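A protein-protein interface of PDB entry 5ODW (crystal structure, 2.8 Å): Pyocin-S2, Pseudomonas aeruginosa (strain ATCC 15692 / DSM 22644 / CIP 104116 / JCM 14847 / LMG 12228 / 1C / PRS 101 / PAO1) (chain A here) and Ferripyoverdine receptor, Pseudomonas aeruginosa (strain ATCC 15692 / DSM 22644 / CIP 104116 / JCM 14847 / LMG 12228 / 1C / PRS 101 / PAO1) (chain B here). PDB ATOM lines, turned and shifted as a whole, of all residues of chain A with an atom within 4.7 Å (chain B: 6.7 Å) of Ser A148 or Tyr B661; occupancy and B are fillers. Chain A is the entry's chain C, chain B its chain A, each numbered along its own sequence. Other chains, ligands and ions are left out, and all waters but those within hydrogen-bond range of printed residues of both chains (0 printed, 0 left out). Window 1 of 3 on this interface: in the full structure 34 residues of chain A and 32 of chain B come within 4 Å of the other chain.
The backbone NH of Tyr B663 lies within hydrogen-bond range of the backbone carbonyl oxygen of Arg B601 (2.8 Å).
The side-chain carboxylate of Glu B646 lies close to the side-chain hydroxyl of Tyr B661, 3.2 Å away.
NH2 of Arg A149 lies within hydrogen-bond range of O of Val A39 (3.4 Å).
The backbone carbonyl oxygen (O) of Gln A144 is in hydrogen-bond range of the side-chain hydroxyl (OG) of Ser A148, at 2.6 Å.
The guanidinium group of Arg A149 is in hydrogen-bond range of the side-chain hydroxyl of Tyr B600.
The side-chain carboxylate of Glu B646 is in salt-bridge range of the side-chain amino group of Lys A150 (2.8 Å).
The side-chain hydroxyl (OH) of Tyr B661 sits close to the side-chain amino group (NZ) of Lys A150 (3.4 Å).
The side-chain hydroxyl (OH) of Tyr B663 sits at hydrogen-bond distance from the backbone carbonyl oxygen (O) of Ala A147.
Of the 14 printed residues of chain B, 6 touch a printed residue of chain A.
Hydrophobic or aromatic side chains of chain A within 4 Å of the printed part of chain B: Leu A146 and Ala A147.
Among the printed residues, Asp or Glu carboxylates within 4 Å of a Lys or Arg side-chain nitrogen of the other chain: Lys A150 with Glu B646 (2.8 Å).
Ser A148 touches one residue of chain B.
Of the printed residues of chain B, Lys A150 touches Glu B646 and Tyr B661.
Phe A155 touches none of the printed residues of chain B.
Of the printed residues of chain A, Trp B599 touches Leu A146 (3.7 Å) and Ala A147 (3.4 Å).
Of the printed residues of chain A, Tyr B600 touches Arg A149.
Pro B654 touches none of the printed residues of chain A.
Of the printed residues of chain A, Thr B660 touches Gln A144.
Of chain A, only Ala A147, Ser A148 and Lys A150 come within 4 Å of Tyr B661.
Printed residues of chain A within 4 Å of Tyr B663: Ala A147 and Arg A149.
The nearest residue of chain B that does not touch Ser A148 is Tyr B663 (4.04 Å).
The nearest residue of chain A that does not touch Tyr B661 is Phe A155 (4.04 Å).
Among the printed residues, merely in contact across the chains: Gln A144 with Thr B660 (3.9 Å), Leu A146 with Trp B599 (3.7 Å), Ala A147 with Trp B599 (3.4 Å), Ala A147 with Tyr B661 (3.8 Å), Ser A148 with Tyr B661 (3.4 Å) and Arg A149 with Tyr B663 (3.8 Å).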
ATOM      1  N   VAL A  39      11.440 -18.238   1.824  1.00  0.00           N
ATOM      2  CA  VAL A  39      10.319 -18.206   0.903  1.00  0.00           C
ATOM      3  C   VAL A  39       9.159 -17.524   1.604  1.00  0.00           C
ATOM      4  O   VAL A  39       8.801 -17.904   2.712  1.00  0.00           O
ATOM      5  CB  VAL A  39       9.898 -19.614   0.479  1.00  0.00           C
ATOM      6  CG1 VAL A  39       8.740 -19.540  -0.499  1.00  0.00           C
ATOM      7  CG2 VAL A  39      11.075 -20.351  -0.133  1.00  0.00           C
ATOM      8  N   GLN A 144       4.272 -30.157  -5.229  1.00  0.00           N
ATOM      9  CA  GLN A 144       5.559 -29.491  -5.026  1.00  0.00           C
ATOM     10  C   GLN A 144       5.421 -27.978  -5.129  1.00  0.00           C
ATOM     11  O   GLN A 144       5.998 -27.285  -4.301  1.00  0.00           O
ATOM     12  CB  GLN A 144       6.603 -30.008  -6.008  1.00  0.00           C
ATOM     13  CG  GLN A 144       7.158 -31.348  -5.596  1.00  0.00           C
ATOM     14  CD  GLN A 144       8.048 -31.957  -6.627  1.00  0.00           C
ATOM     15  OE1 GLN A 144       7.655 -32.155  -7.772  1.00  0.00           O
ATOM     16  NE2 GLN A 144       9.259 -32.316  -6.222  1.00  0.00           N
ATOM     17  N   LEU A 145       4.623 -27.467  -6.099  1.00  0.00           N
ATOM     18  CA  LEU A 145       4.368 -26.021  -6.262  1.00  0.00           C
ATOM     19  C   LEU A 145       3.622 -25.449  -5.050  1.00  0.00           C
ATOM     20  O   LEU A 145       4.011 -24.401  -4.528  1.00  0.00           O
ATOM     21  CB  LEU A 145       3.589 -25.705  -7.566  1.00  0.00           C
ATOM     22  CG  LEU A 145       4.280 -25.930  -8.944  1.00  0.00           C
ATOM     23  CD1 LEU A 145       3.490 -25.289 -10.039  1.00  0.00           C
ATOM     24  CD2 LEU A 145       5.691 -25.373  -8.987  1.00  0.00           C
ATOM     25  N   LEU A 146       2.563 -26.159  -4.602  1.00  0.00           N
ATOM     26  CA  LEU A 146       1.711 -25.806  -3.453  1.00  0.00           C
ATOM     27  C   LEU A 146       2.477 -25.852  -2.116  1.00  0.00           C
ATOM     28  O   LEU A 146       2.358 -24.925  -1.318  1.00  0.00           O
ATOM     29  CB  LEU A 146       0.454 -26.695  -3.415  1.00  0.00           C
ATOM     30  CG  LEU A 146      -0.600 -26.446  -4.513  1.00  0.00           C
ATOM     31  CD1 LEU A 146      -1.434 -27.667  -4.745  1.00  0.00           C
ATOM     32  CD2 LEU A 146      -1.518 -25.330  -4.156  1.00  0.00           C
ATOM     33  N   ALA A 147       3.307 -26.889  -1.911  1.00  0.00           N
ATOM     34  CA  ALA A 147       4.148 -27.071  -0.719  1.00  0.00           C
ATOM     35  C   ALA A 147       5.311 -26.093  -0.646  1.00  0.00           C
ATOM     36  O   ALA A 147       5.557 -25.557   0.425  1.00  0.00           O
ATOM     37  CB  ALA A 147       4.682 -28.492  -0.658  1.00  0.00           C
ATOM     38  N   SER A 148       6.038 -25.868  -1.760  1.00  0.00           N
ATOM     39  CA  SER A 148       7.210 -24.989  -1.778  1.00  0.00           C
ATOM     40  C   SER A 148       6.912 -23.504  -1.870  1.00  0.00           C
ATOM     41  O   SER A 148       7.733 -22.711  -1.436  1.00  0.00           O
ATOM     42  CB  SER A 148       8.175 -25.388  -2.891  1.00  0.00           C
ATOM     43  OG  SER A 148       7.627 -25.199  -4.185  1.00  0.00           O
ATOM     44  N   ARG A 149       5.777 -23.120  -2.477  1.00  0.00           N
ATOM     45  CA  ARG A 149       5.342 -21.726  -2.735  1.00  0.00           C
ATOM     46  C   ARG A 149       6.337 -20.957  -3.618  1.00  0.00           C
ATOM     47  O   ARG A 149       6.172 -19.748  -3.814  1.00  0.00           O
ATOM     48  CB  ARG A 149       5.048 -20.911  -1.460  1.00  0.00           C
ATOM     49  CG  ARG A 149       4.196 -21.568  -0.414  1.00  0.00           C
ATOM     50  CD  ARG A 149       4.134 -20.734   0.846  1.00  0.00           C
ATOM     51  NE  ARG A 149       5.442 -20.477   1.452  1.00  0.00           N
ATOM     52  CZ  ARG A 149       6.127 -21.344   2.191  1.00  0.00           C
ATOM     53  NH1 ARG A 149       5.653 -22.567   2.404  1.00  0.00           N
ATOM     54  NH2 ARG A 149       7.297 -21.001   2.712  1.00  0.00           N
ATOM     55  N   LYS A 150       7.364 -21.652  -4.145  1.00  0.00           N
ATOM     56  CA  LYS A 150       8.392 -21.042  -4.984  1.00  0.00           C
ATOM     57  C   LYS A 150       8.157 -21.247  -6.484  1.00  0.00           C
ATOM     58  O   LYS A 150       7.177 -21.875  -6.896  1.00  0.00           O
ATOM     59  CB  LYS A 150       9.811 -21.468  -4.559  1.00  0.00           C
ATOM     60  CG  LYS A 150      10.125 -22.955  -4.585  1.00  0.00           C
ATOM     61  CD  LYS A 150      11.399 -23.214  -3.782  1.00  0.00           C
ATOM     62  CE  LYS A 150      11.970 -24.584  -4.018  1.00  0.00           C
ATOM     63  NZ  LYS A 150      13.312 -24.711  -3.417  1.00  0.00           N
ATOM     64  N   PHE A 155      11.255 -27.282 -10.850  1.00  0.00           N
ATOM     65  CA  PHE A 155      10.366 -28.442 -10.772  1.00  0.00           C
ATOM     66  C   PHE A 155      10.017 -28.946 -12.146  1.00  0.00           C
ATOM     67  O   PHE A 155      10.151 -30.152 -12.403  1.00  0.00           O
ATOM     68  CB  PHE A 155       9.076 -28.103  -9.992  1.00  0.00           C
ATOM     69  CG  PHE A 155       9.364 -27.644  -8.592  1.00  0.00           C
ATOM     70  CD1 PHE A 155       9.764 -28.554  -7.612  1.00  0.00           C
ATOM     71  CD2 PHE A 155       9.298 -26.297  -8.260  1.00  0.00           C
ATOM     72  CE1 PHE A 155      10.073 -28.124  -6.318  1.00  0.00           C
ATOM     73  CE2 PHE A 155       9.599 -25.868  -6.962  1.00  0.00           C
ATOM     74  CZ  PHE A 155       9.978 -26.786  -5.999  1.00  0.00           C
ATOM     75  N   TRP B 599       1.674 -28.946   5.662  1.00  0.00           N
ATOM     76  CA  TRP B 599       2.607 -28.931   4.538  1.00  0.00           C
ATOM     77  C   TRP B 599       4.056 -29.079   5.026  1.00  0.00           C
ATOM     78  O   TRP B 599       4.886 -29.655   4.319  1.00  0.00           O
ATOM     79  CB  TRP B 599       2.423 -27.677   3.664  1.00  0.00           C
ATOM     80  CG  TRP B 599       1.147 -27.662   2.864  1.00  0.00           C
ATOM     81  CD1 TRP B 599      -0.017 -27.038   3.202  1.00  0.00           C
ATOM     82  CD2 TRP B 599       0.910 -28.287   1.593  1.00  0.00           C
ATOM     83  NE1 TRP B 599      -0.967 -27.248   2.233  1.00  0.00           N
ATOM     84  CE2 TRP B 599      -0.418 -27.989   1.219  1.00  0.00           C
ATOM     85  CE3 TRP B 599       1.674 -29.104   0.753  1.00  0.00           C
ATOM     86  CZ2 TRP B 599      -0.987 -28.452   0.025  1.00  0.00           C
ATOM     87  CZ3 TRP B 599       1.117 -29.541  -0.444  1.00  0.00           C
ATOM     88  CH2 TRP B 599      -0.208 -29.238  -0.783  1.00  0.00           C
ATOM     89  N   TYR B 600       4.336 -28.595   6.258  1.00  0.00           N
ATOM     90  CA  TYR B 600       5.642 -28.635   6.911  1.00  0.00           C
ATOM     91  C   TYR B 600       5.870 -29.966   7.648  1.00  0.00           C
ATOM     92  O   TYR B 600       5.747 -30.035   8.869  1.00  0.00           O
ATOM     93  CB  TYR B 600       5.808 -27.435   7.856  1.00  0.00           C
ATOM     94  CG  TYR B 600       5.789 -26.087   7.172  1.00  0.00           C
ATOM     95  CD1 TYR B 600       4.600 -25.406   6.968  1.00  0.00           C
ATOM     96  CD2 TYR B 600       6.964 -25.483   6.751  1.00  0.00           C
ATOM     97  CE1 TYR B 600       4.577 -24.156   6.349  1.00  0.00           C
ATOM     98  CE2 TYR B 600       6.960 -24.229   6.153  1.00  0.00           C
ATOM     99  CZ  TYR B 600       5.766 -23.565   5.953  1.00  0.00           C
ATOM    100  OH  TYR B 600       5.781 -22.316   5.381  1.00  0.00           O
ATOM    101  N   ARG B 601       6.206 -31.026   6.895  1.00  0.00           N
ATOM    102  CA  ARG B 601       6.487 -32.371   7.419  1.00  0.00           C
ATOM    103  C   ARG B 601       7.868 -32.781   6.941  1.00  0.00           C
ATOM    104  O   ARG B 601       8.335 -32.236   5.940  1.00  0.00           O
ATOM    105  CB  ARG B 601       5.438 -33.384   6.930  1.00  0.00           C
ATOM    106  CG  ARG B 601       3.996 -33.015   7.228  1.00  0.00           C
ATOM    107  CD  ARG B 601       3.010 -33.899   6.509  1.00  0.00           C
ATOM    108  NE  ARG B 601       1.684 -33.723   7.094  1.00  0.00           N
ATOM    109  CZ  ARG B 601       1.126 -34.555   7.973  1.00  0.00           C
ATOM    110  NH1 ARG B 601       1.752 -35.667   8.342  1.00  0.00           N
ATOM    111  NH2 ARG B 601      -0.074 -34.301   8.460  1.00  0.00           N
ATOM    112  N   ASP B 602       8.504 -33.693   7.667  1.00  0.00           N
ATOM    113  CA  ASP B 602       9.830 -34.194   7.335  1.00  0.00           C
ATOM    114  C   ASP B 602       9.748 -35.330   6.335  1.00  0.00           C
ATOM    115  O   ASP B 602       8.676 -35.656   5.842  1.00  0.00           O
ATOM    116  CB  ASP B 602      10.575 -34.641   8.586  1.00  0.00           C
ATOM    117  CG  ASP B 602       9.892 -35.779   9.291  1.00  0.00           C
ATOM    118  OD1 ASP B 602       8.970 -36.371   8.705  1.00  0.00           O
ATOM    119  OD2 ASP B 602      10.277 -36.082  10.433  1.00  0.00           O
ATOM    120  N   GLU B 646      13.945 -25.917   4.017  1.00  0.00           N
ATOM    121  CA  GLU B 646      13.781 -26.941   2.998  1.00  0.00           C
ATOM    122  C   GLU B 646      14.828 -28.041   3.108  1.00  0.00           C
ATOM    123  O   GLU B 646      16.008 -27.766   3.308  1.00  0.00           O
ATOM    124  CB  GLU B 646      13.861 -26.292   1.619  1.00  0.00           C
ATOM    125  CG  GLU B 646      14.035 -27.260   0.467  1.00  0.00           C
ATOM    126  CD  GLU B 646      14.379 -26.552  -0.818  1.00  0.00           C
ATOM    127  OE1 GLU B 646      14.331 -25.309  -0.834  1.00  0.00           O
ATOM    128  OE2 GLU B 646      14.700 -27.234  -1.808  1.00  0.00           O
ATOM    129  N   ASP B 647      14.395 -29.291   2.975  1.00  0.00           N
ATOM    130  CA  ASP B 647      15.316 -30.416   3.014  1.00  0.00           C
ATOM    131  C   ASP B 647      15.733 -30.636   1.569  1.00  0.00           C
ATOM    132  O   ASP B 647      15.104 -31.392   0.840  1.00  0.00           O
ATOM    133  CB  ASP B 647      14.606 -31.651   3.562  1.00  0.00           C
ATOM    134  CG  ASP B 647      15.559 -32.662   4.155  1.00  0.00           C
ATOM    135  OD1 ASP B 647      16.776 -32.555   3.919  1.00  0.00           O
ATOM    136  OD2 ASP B 647      15.080 -33.568   4.858  1.00  0.00           O
ATOM    137  N   TYR B 650      16.740 -34.473   0.504  1.00  0.00           N
ATOM    138  CA  TYR B 650      15.552 -35.291   0.275  1.00  0.00           C
ATOM    139  C   TYR B 650      14.778 -34.821  -0.938  1.00  0.00           C
ATOM    140  O   TYR B 650      14.466 -35.632  -1.792  1.00  0.00           O
ATOM    141  CB  TYR B 650      14.615 -35.338   1.497  1.00  0.00           C
ATOM    142  CG  TYR B 650      13.355 -36.140   1.228  1.00  0.00           C
ATOM    143  CD1 TYR B 650      13.341 -37.525   1.369  1.00  0.00           C
ATOM    144  CD2 TYR B 650      12.184 -35.518   0.793  1.00  0.00           C
ATOM    145  CE1 TYR B 650      12.193 -38.272   1.096  1.00  0.00           C
ATOM    146  CE2 TYR B 650      11.030 -36.257   0.510  1.00  0.00           C
ATOM    147  CZ  TYR B 650      11.044 -37.633   0.659  1.00  0.00           C
ATOM    148  OH  TYR B 650       9.929 -38.368   0.372  1.00  0.00           O
ATOM    149  N   ASN B 651      14.448 -33.522  -1.003  1.00  0.00           N
ATOM    150  CA  ASN B 651      13.653 -32.913  -2.073  1.00  0.00           C
ATOM    151  C   ASN B 651      14.218 -33.057  -3.479  1.00  0.00           C
ATOM    152  O   ASN B 651      13.441 -33.038  -4.439  1.00  0.00           O
ATOM    153  CB  ASN B 651      13.379 -31.458  -1.763  1.00  0.00           C
ATOM    154  CG  ASN B 651      12.450 -31.281  -0.597  1.00  0.00           C
ATOM    155  OD1 ASN B 651      11.835 -32.222  -0.078  1.00  0.00           O
ATOM    156  ND2 ASN B 651      12.317 -30.062  -0.168  1.00  0.00           N
ATOM    157  N   PRO B 654      13.430 -37.373  -3.883  1.00  0.00           N
ATOM    158  CA  PRO B 654      12.424 -37.870  -2.916  1.00  0.00           C
ATOM    159  C   PRO B 654      12.197 -39.374  -2.990  1.00  0.00           C
ATOM    160  O   PRO B 654      12.008 -39.890  -4.080  1.00  0.00           O
ATOM    161  CB  PRO B 654      11.158 -37.066  -3.259  1.00  0.00           C
ATOM    162  CG  PRO B 654      11.343 -36.622  -4.655  1.00  0.00           C
ATOM    163  CD  PRO B 654      12.817 -36.451  -4.866  1.00  0.00           C
ATOM    164  N   ILE B 659       5.207 -38.201   0.949  1.00  0.00           N
ATOM    165  CA  ILE B 659       5.741 -36.852   0.977  1.00  0.00           C
ATOM    166  C   ILE B 659       6.569 -36.624  -0.290  1.00  0.00           C
ATOM    167  O   ILE B 659       7.482 -37.391  -0.581  1.00  0.00           O
ATOM    168  CB  ILE B 659       6.627 -36.641   2.220  1.00  0.00           C
ATOM    169  CG1 ILE B 659       6.864 -35.154   2.474  1.00  0.00           C
ATOM    170  CG2 ILE B 659       7.942 -37.390   2.083  1.00  0.00           C
ATOM    171  CD1 ILE B 659       5.674 -34.440   3.069  1.00  0.00           C
ATOM    172  N   THR B 660       6.259 -35.569  -1.033  1.00  0.00           N
ATOM    173  CA  THR B 660       6.984 -35.229  -2.260  1.00  0.00           C
ATOM    174  C   THR B 660       7.958 -34.020  -2.041  1.00  0.00           C
ATOM    175  O   THR B 660       9.001 -33.930  -2.703  1.00  0.00           O
ATOM    176  CB  THR B 660       5.993 -35.075  -3.427  1.00  0.00           C
ATOM    177  OG1 THR B 660       5.069 -34.063  -3.106  1.00  0.00           O
ATOM    178  CG2 THR B 660       5.249 -36.375  -3.775  1.00  0.00           C
ATOM    179  N   TYR B 661       7.601 -33.119  -1.110  1.00  0.00           N
ATOM    180  CA  TYR B 661       8.372 -31.939  -0.700  1.00  0.00           C
ATOM    181  C   TYR B 661       8.391 -31.900   0.837  1.00  0.00           C
ATOM    182  O   TYR B 661       7.352 -31.697   1.471  1.00  0.00           O
ATOM    183  CB  TYR B 661       7.775 -30.656  -1.317  1.00  0.00           C
ATOM    184  CG  TYR B 661       8.694 -29.450  -1.273  1.00  0.00           C
ATOM    185  CD1 TYR B 661       9.625 -29.221  -2.284  1.00  0.00           C
ATOM    186  CD2 TYR B 661       8.620 -28.527  -0.231  1.00  0.00           C
ATOM    187  CE1 TYR B 661      10.500 -28.138  -2.227  1.00  0.00           C
ATOM    188  CE2 TYR B 661       9.483 -27.434  -0.168  1.00  0.00           C
ATOM    189  CZ  TYR B 661      10.418 -27.243  -1.169  1.00  0.00           C
ATOM    190  OH  TYR B 661      11.231 -26.139  -1.129  1.00  0.00           O
ATOM    191  N   ALA B 662       9.549 -32.193   1.425  1.00  0.00           N
ATOM    192  CA  ALA B 662       9.749 -32.277   2.870  1.00  0.00           C
ATOM    193  C   ALA B 662      10.559 -31.117   3.411  1.00  0.00           C
ATOM    194  O   ALA B 662      11.144 -30.367   2.634  1.00  0.00           O
ATOM    195  CB  ALA B 662      10.423 -33.586   3.236  1.00  0.00           C
ATOM    196  N   TYR B 663      10.567 -30.971   4.754  1.00  0.00           N
ATOM    197  CA  TYR B 663      11.245 -29.929   5.536  1.00  0.00           C
ATOM    198  C   TYR B 663      12.146 -30.512   6.661  1.00  0.00           C
ATOM    199  O   TYR B 663      12.065 -31.699   7.022  1.00  0.00           O
ATOM    200  CB  TYR B 663      10.231 -28.933   6.098  1.00  0.00           C
ATOM    201  CG  TYR B 663       9.562 -28.093   5.043  1.00  0.00           C
ATOM    202  CD1 TYR B 663       8.461 -28.568   4.340  1.00  0.00           C
ATOM    203  CD2 TYR B 663       9.989 -26.789   4.786  1.00  0.00           C
ATOM    204  CE1 TYR B 663       7.832 -27.785   3.372  1.00  0.00           C
ATOM    205  CE2 TYR B 663       9.363 -25.996   3.823  1.00  0.00           C
ATOM    206  CZ  TYR B 663       8.289 -26.502   3.114  1.00  0.00           C
ATOM    207  OH  TYR B 663       7.667 -25.738   2.163  1.00  0.00           O
